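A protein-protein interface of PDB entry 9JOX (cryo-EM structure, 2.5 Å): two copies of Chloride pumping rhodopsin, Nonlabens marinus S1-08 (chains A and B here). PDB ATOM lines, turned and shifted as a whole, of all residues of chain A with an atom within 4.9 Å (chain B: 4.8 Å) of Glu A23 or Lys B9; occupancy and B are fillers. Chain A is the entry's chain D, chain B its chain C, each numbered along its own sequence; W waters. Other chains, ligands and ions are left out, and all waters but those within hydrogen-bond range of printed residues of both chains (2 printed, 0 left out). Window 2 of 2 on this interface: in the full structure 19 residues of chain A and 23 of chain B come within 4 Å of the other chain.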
ATOM      1  N   SER A  18       2.371  25.652  24.771  1.00  0.00           N
ATOM      2  CA  SER A  18       2.827  24.313  25.076  1.00  0.00           C
ATOM      3  C   SER A  18       1.656  23.414  25.457  1.00  0.00           C
ATOM      4  O   SER A  18       0.710  23.886  26.097  1.00  0.00           O
ATOM      5  CB  SER A  18       3.801  24.371  26.198  1.00  0.00           C
ATOM      6  OG  SER A  18       3.172  24.458  27.463  1.00  0.00           O
ATOM      7  N   ALA A  19       1.791  22.105  25.187  1.00  0.00           N
ATOM      8  CA  ALA A  19       0.799  21.134  25.634  1.00  0.00           C
ATOM      9  C   ALA A  19       0.459  21.302  27.120  1.00  0.00           C
ATOM     10  O   ALA A  19      -0.710  21.243  27.500  1.00  0.00           O
ATOM     11  CB  ALA A  19       1.326  19.758  25.372  1.00  0.00           C
ATOM     12  N   GLY A  20       1.478  21.598  27.940  1.00  0.00           N
ATOM     13  CA  GLY A  20       1.273  21.740  29.367  1.00  0.00           C
ATOM     14  C   GLY A  20       0.437  22.969  29.719  1.00  0.00           C
ATOM     15  O   GLY A  20      -0.557  22.856  30.432  1.00  0.00           O
ATOM     16  N   GLN A  21       0.846  24.128  29.208  1.00  0.00           N
ATOM     17  CA  GLN A  21       0.060  25.333  29.366  1.00  0.00           C
ATOM     18  C   GLN A  21      -1.357  25.134  28.811  1.00  0.00           C
ATOM     19  O   GLN A  21      -2.360  25.386  29.470  1.00  0.00           O
ATOM     20  CB  GLN A  21       0.665  26.481  28.579  1.00  0.00           C
ATOM     21  CG  GLN A  21       2.005  26.938  29.120  1.00  0.00           C
ATOM     22  CD  GLN A  21       2.643  27.980  28.227  1.00  0.00           C
ATOM     23  OE1 GLN A  21       2.746  27.809  27.001  1.00  0.00           O
ATOM     24  NE2 GLN A  21       3.028  29.092  28.832  1.00  0.00           N
ATOM     25  N   PHE A  22      -1.447  24.660  27.594  1.00  0.00           N
ATOM     26  CA  PHE A  22      -2.743  24.500  27.003  1.00  0.00           C
ATOM     27  C   PHE A  22      -3.593  23.555  27.828  1.00  0.00           C
ATOM     28  O   PHE A  22      -4.791  23.828  27.996  1.00  0.00           O
ATOM     29  CB  PHE A  22      -2.652  24.018  25.566  1.00  0.00           C
ATOM     30  CG  PHE A  22      -4.011  23.996  24.924  1.00  0.00           C
ATOM     31  CD1 PHE A  22      -4.560  25.145  24.398  1.00  0.00           C
ATOM     32  CD2 PHE A  22      -4.737  22.828  24.895  1.00  0.00           C
ATOM     33  CE1 PHE A  22      -5.802  25.082  23.821  1.00  0.00           C
ATOM     34  CE2 PHE A  22      -5.971  22.785  24.311  1.00  0.00           C
ATOM     35  CZ  PHE A  22      -6.499  23.889  23.811  1.00  0.00           C
ATOM     36  N   GLU A  23      -3.013  22.457  28.325  1.00  0.00           N
ATOM     37  CA  GLU A  23      -3.847  21.480  29.028  1.00  0.00           C
ATOM     38  C   GLU A  23      -4.267  22.024  30.407  1.00  0.00           C
ATOM     39  O   GLU A  23      -5.402  21.850  30.817  1.00  0.00           O
ATOM     40  CB  GLU A  23      -3.183  20.123  29.150  1.00  0.00           C
ATOM     41  CG  GLU A  23      -3.031  19.366  27.842  1.00  0.00           C
ATOM     42  CD  GLU A  23      -2.067  18.172  27.943  1.00  0.00           C
ATOM     43  OE1 GLU A  23      -1.271  18.074  28.923  1.00  0.00           O
ATOM     44  OE2 GLU A  23      -2.130  17.294  27.041  1.00  0.00           O
ATOM     45  N   PHE A  24      -3.366  22.750  31.079  1.00  0.00           N
ATOM     46  CA  PHE A  24      -3.652  23.352  32.368  1.00  0.00           C
ATOM     47  C   PHE A  24      -4.906  24.230  32.289  1.00  0.00           C
ATOM     48  O   PHE A  24      -5.877  24.048  33.034  1.00  0.00           O
ATOM     49  CB  PHE A  24      -2.470  24.202  32.832  1.00  0.00           C
ATOM     50  CG  PHE A  24      -2.554  24.733  34.250  1.00  0.00           C
ATOM     51  CD1 PHE A  24      -2.913  23.891  35.292  1.00  0.00           C
ATOM     52  CD2 PHE A  24      -2.373  26.093  34.512  1.00  0.00           C
ATOM     53  CE1 PHE A  24      -3.095  24.392  36.583  1.00  0.00           C
ATOM     54  CE2 PHE A  24      -2.544  26.589  35.793  1.00  0.00           C
ATOM     55  CZ  PHE A  24      -2.920  25.738  36.821  1.00  0.00           C
ATOM     56  N   ILE A  25      -4.900  25.155  31.340  1.00  0.00           N
ATOM     57  CA  ILE A  25      -6.049  26.022  31.160  1.00  0.00           C
ATOM     58  C   ILE A  25      -7.309  25.207  30.873  1.00  0.00           C
ATOM     59  O   ILE A  25      -8.343  25.489  31.455  1.00  0.00           O
ATOM     60  CB  ILE A  25      -5.770  27.049  30.058  1.00  0.00           C
ATOM     61  CG1 ILE A  25      -4.789  28.107  30.542  1.00  0.00           C
ATOM     62  CG2 ILE A  25      -7.076  27.656  29.593  1.00  0.00           C
ATOM     63  CD1 ILE A  25      -4.245  28.957  29.422  1.00  0.00           C
ATOM     64  N   ASP A  26      -7.237  24.147  30.069  1.00  0.00           N
ATOM     65  CA  ASP A  26      -8.440  23.355  29.855  1.00  0.00           C
ATOM     66  C   ASP A  26      -8.885  22.664  31.155  1.00  0.00           C
ATOM     67  O   ASP A  26     -10.085  22.516  31.394  1.00  0.00           O
ATOM     68  CB  ASP A  26      -8.296  22.343  28.729  1.00  0.00           C
ATOM     69  CG  ASP A  26      -9.638  21.874  28.175  1.00  0.00           C
ATOM     70  OD1 ASP A  26     -10.622  22.671  28.205  1.00  0.00           O
ATOM     71  OD2 ASP A  26      -9.721  20.698  27.733  1.00  0.00           O
ATOM     72  N   HIS A  27      -7.933  22.251  31.995  1.00  0.00           N
ATOM     73  CA  HIS A  27      -8.254  21.668  33.282  1.00  0.00           C
ATOM     74  C   HIS A  27      -8.964  22.687  34.176  1.00  0.00           C
ATOM     75  O   HIS A  27      -9.977  22.358  34.782  1.00  0.00           O
ATOM     76  CB  HIS A  27      -7.027  21.098  34.004  1.00  0.00           C
ATOM     77  CG  HIS A  27      -6.293  20.058  33.255  1.00  0.00           C
ATOM     78  ND1 HIS A  27      -6.819  19.275  32.232  1.00  0.00           N
ATOM     79  CD2 HIS A  27      -4.986  19.728  33.381  1.00  0.00           C
ATOM     80  CE1 HIS A  27      -5.834  18.480  31.773  1.00  0.00           C
ATOM     81  NE2 HIS A  27      -4.732  18.695  32.484  1.00  0.00           N
ATOM     82  N   MET B   8       4.637  16.672  25.137  1.00  0.00           N
ATOM     83  CA  MET B   8       3.706  15.638  25.689  1.00  0.00           C
ATOM     84  C   MET B   8       3.959  15.423  27.177  1.00  0.00           C
ATOM     85  O   MET B   8       5.107  15.326  27.605  1.00  0.00           O
ATOM     86  CB  MET B   8       3.884  14.274  25.009  1.00  0.00           C
ATOM     87  CG  MET B   8       2.700  13.847  24.191  1.00  0.00           C
ATOM     88  SD  MET B   8       1.895  15.257  23.407  1.00  0.00           S
ATOM     89  CE  MET B   8       1.543  14.508  21.816  1.00  0.00           C
ATOM     90  N   LYS B   9       2.879  15.341  27.947  1.00  0.00           N
ATOM     91  CA  LYS B   9       3.001  15.288  29.395  1.00  0.00           C
ATOM     92  C   LYS B   9       2.555  13.927  29.926  1.00  0.00           C
ATOM     93  O   LYS B   9       2.993  13.480  30.975  1.00  0.00           O
ATOM     94  CB  LYS B   9       2.132  16.362  30.057  1.00  0.00           C
ATOM     95  CG  LYS B   9       2.221  17.772  29.507  1.00  0.00           C
ATOM     96  CD  LYS B   9       3.591  18.438  29.536  1.00  0.00           C
ATOM     97  CE  LYS B   9       4.014  18.854  30.867  1.00  0.00           C
ATOM     98  NZ  LYS B   9       5.411  19.302  30.801  1.00  0.00           N
ATOM     99  N   ASN B  10       1.620  13.294  29.231  1.00  0.00           N
ATOM    100  CA  ASN B  10       1.030  12.060  29.684  1.00  0.00           C
ATOM    101  C   ASN B  10       1.400  10.964  28.699  1.00  0.00           C
ATOM    102  O   ASN B  10       1.375  11.177  27.495  1.00  0.00           O
ATOM    103  CB  ASN B  10      -0.468  12.262  29.889  1.00  0.00           C
ATOM    104  CG  ASN B  10      -0.851  12.761  31.275  1.00  0.00           C
ATOM    105  OD1 ASN B  10      -2.007  12.612  31.680  1.00  0.00           O
ATOM    106  ND2 ASN B  10       0.067  13.330  32.044  1.00  0.00           N
ATOM    107  N   ILE B  11       1.651   9.762  29.217  1.00  0.00           N
ATOM    108  CA  ILE B  11       1.956   8.620  28.373  1.00  0.00           C
ATOM    109  C   ILE B  11       0.748   8.150  27.555  1.00  0.00           C
ATOM    110  O   ILE B  11       0.910   7.357  26.635  1.00  0.00           O
ATOM    111  CB  ILE B  11       2.542   7.461  29.197  1.00  0.00           C
ATOM    112  CG1 ILE B  11       1.517   6.733  30.008  1.00  0.00           C
ATOM    113  CG2 ILE B  11       3.699   7.937  30.067  1.00  0.00           C
ATOM    114  CD1 ILE B  11       2.048   5.426  30.557  1.00  0.00           C
ATOM    115  N   THR B  96      -4.560  16.469  22.241  1.00  0.00           N
ATOM    116  CA  THR B  96      -3.858  15.535  23.117  1.00  0.00           C
ATOM    117  C   THR B  96      -4.813  15.095  24.228  1.00  0.00           C
ATOM    118  O   THR B  96      -5.846  15.717  24.420  1.00  0.00           O
ATOM    119  CB  THR B  96      -2.568  16.150  23.663  1.00  0.00           C
ATOM    120  OG1 THR B  96      -2.890  17.309  24.423  1.00  0.00           O
ATOM    121  CG2 THR B  96      -1.615  16.616  22.580  1.00  0.00           C
ATOM    122  N   PHE B  97      -4.474  14.004  24.917  1.00  0.00           N
ATOM    123  CA  PHE B  97      -5.283  13.477  26.004  1.00  0.00           C
ATOM    124  C   PHE B  97      -4.456  13.494  27.288  1.00  0.00           C
ATOM    125  O   PHE B  97      -3.299  13.087  27.278  1.00  0.00           O
ATOM    126  CB  PHE B  97      -5.781  12.093  25.591  1.00  0.00           C
ATOM    127  CG  PHE B  97      -6.736  11.489  26.602  1.00  0.00           C
ATOM    128  CD1 PHE B  97      -8.106  11.690  26.468  1.00  0.00           C
ATOM    129  CD2 PHE B  97      -6.281  10.754  27.683  1.00  0.00           C
ATOM    130  CE1 PHE B  97      -9.011  11.146  27.386  1.00  0.00           C
ATOM    131  CE2 PHE B  97      -7.203  10.261  28.634  1.00  0.00           C
ATOM    132  CZ  PHE B  97      -8.546  10.473  28.487  1.00  0.00           C
ATOM    133  N   SER B  98      -5.051  13.979  28.395  1.00  0.00           N
ATOM    134  CA  SER B  98      -4.408  13.980  29.710  1.00  0.00           C
ATOM    135  C   SER B  98      -5.374  13.522  30.807  1.00  0.00           C
ATOM    136  O   SER B  98      -6.579  13.459  30.580  1.00  0.00           O
ATOM    137  CB  SER B  98      -3.835  15.334  30.053  1.00  0.00           C
ATOM    138  OG  SER B  98      -4.740  16.415  29.823  1.00  0.00           O
ATOM    139  N   GLN B 150       2.813  14.629  38.126  1.00  0.00           N
ATOM    140  CA  GLN B 150       2.390  13.824  36.980  1.00  0.00           C
ATOM    141  C   GLN B 150       2.741  14.538  35.678  1.00  0.00           C
ATOM    142  O   GLN B 150       2.670  13.928  34.622  1.00  0.00           O
ATOM    143  CB  GLN B 150       0.918  13.365  36.997  1.00  0.00           C
ATOM    144  CG  GLN B 150      -0.112  14.481  37.101  1.00  0.00           C
ATOM    145  CD  GLN B 150      -0.503  15.099  35.786  1.00  0.00           C
ATOM    146  OE1 GLN B 150      -0.859  14.372  34.863  1.00  0.00           O
ATOM    147  NE2 GLN B 150      -0.481  16.428  35.705  1.00  0.00           N
ATOM    148  N   LEU B 151       3.129  15.811  35.775  1.00  0.00           N
ATOM    149  CA  LEU B 151       3.786  16.542  34.694  1.00  0.00           C
ATOM    150  C   LEU B 151       5.171  15.997  34.323  1.00  0.00           C
ATOM    151  O   LEU B 151       5.739  16.446  33.342  1.00  0.00           O
ATOM    152  CB  LEU B 151       3.913  18.023  35.050  1.00  0.00           C
ATOM    153  CG  LEU B 151       2.587  18.782  35.130  1.00  0.00           C
ATOM    154  CD1 LEU B 151       2.752  20.235  35.495  1.00  0.00           C
ATOM    155  CD2 LEU B 151       1.794  18.617  33.864  1.00  0.00           C
ATOM    156  N   GLU B 153       5.705  12.549  33.851  1.00  0.00           N
ATOM    157  CA  GLU B 153       5.575  11.113  33.703  1.00  0.00           C
ATOM    158  C   GLU B 153       6.283  10.650  32.428  1.00  0.00           C
ATOM    159  O   GLU B 153       6.714   9.498  32.343  1.00  0.00           O
ATOM    160  CB  GLU B 153       4.147  10.631  33.929  1.00  0.00           C
ATOM    161  CG  GLU B 153       3.153  10.993  32.844  1.00  0.00           C
ATOM    162  CD  GLU B 153       1.810  10.301  33.105  1.00  0.00           C
ATOM    163  OE1 GLU B 153       1.261  10.438  34.223  1.00  0.00           O
ATOM    164  OE2 GLU B 153       1.290   9.622  32.185  1.00  0.00           O
ATOM    165  N   VAL B 154       6.432  11.563  31.465  1.00  0.00           N
ATOM    166  CA  VAL B 154       7.055  11.245  30.191  1.00  0.00           C
ATOM    167  C   VAL B 154       8.546  11.559  30.274  1.00  0.00           C
ATOM    168  O   VAL B 154       9.375  10.708  29.956  1.00  0.00           O
ATOM    169  CB  VAL B 154       6.354  11.992  29.042  1.00  0.00           C
ATOM    170  CG1 VAL B 154       7.064  11.756  27.723  1.00  0.00           C
ATOM    171  CG2 VAL B 154       4.867  11.617  28.910  1.00  0.00           C
HETATM  172  O   HOH W   1      -2.647  16.037  32.656  1.00  0.00           O
HETATM  173  O   HOH W   2      -0.862  14.161  27.314  1.00  0.00           O
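The side-chain carboxylate (OE2) of Glu A23 lies within hydrogen-bond range of the side-chain hydroxyl (OG1) of Thr B96 (2.7 Å).
ND1 of His A27 lies close to O of Glu A23 (3.3 Å).
Among the printed residues, pairs that only touch across the chains: His A27 with Ser B98 (3.0 Å), Glu A23 with Lys B9 (3.6 Å) and Glu A23 with Ser B98 (3.7 Å).
Of the printed residues of chain B, Glu A23 touches Lys B9 (3.6 Å), Thr B96 (2.7 Å) and Ser B98 (3.7 Å). Of the printed residues of chain A, Thr B96 touches Glu A23. Printed residues of chain A within 4 Å of Ser B98: Glu A23 and His A27. Printed residues of chain B within 4 Å of His A27: Ser B98.
Hydrophobic or aromatic side chains of chain A that line the printed part of chain B: His A27. Among the printed residues, 4 pairs touch across the chains. Among the printed residues, no Asp or Glu carboxylate lies within 4 Å of a Lys or Arg side-chain nitrogen of the other chain.
No position is printed for both chains. Of the 4 pairs that touch across the chains among the printed residues, none has its exchanged pair printed and touching as well.
Water W2 lies within hydrogen-bond range of the backbone carbonyl oxygen (O) of Phe B97 (2.7 Å), the backbone NH (N) of Asn B10 (3.3 Å) and the side-chain carboxylate (OE2) of Glu A23 (3.4 Å). Water W1 lies within hydrogen-bond range of OE1 of Gln B150 and NE2 of His A27.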
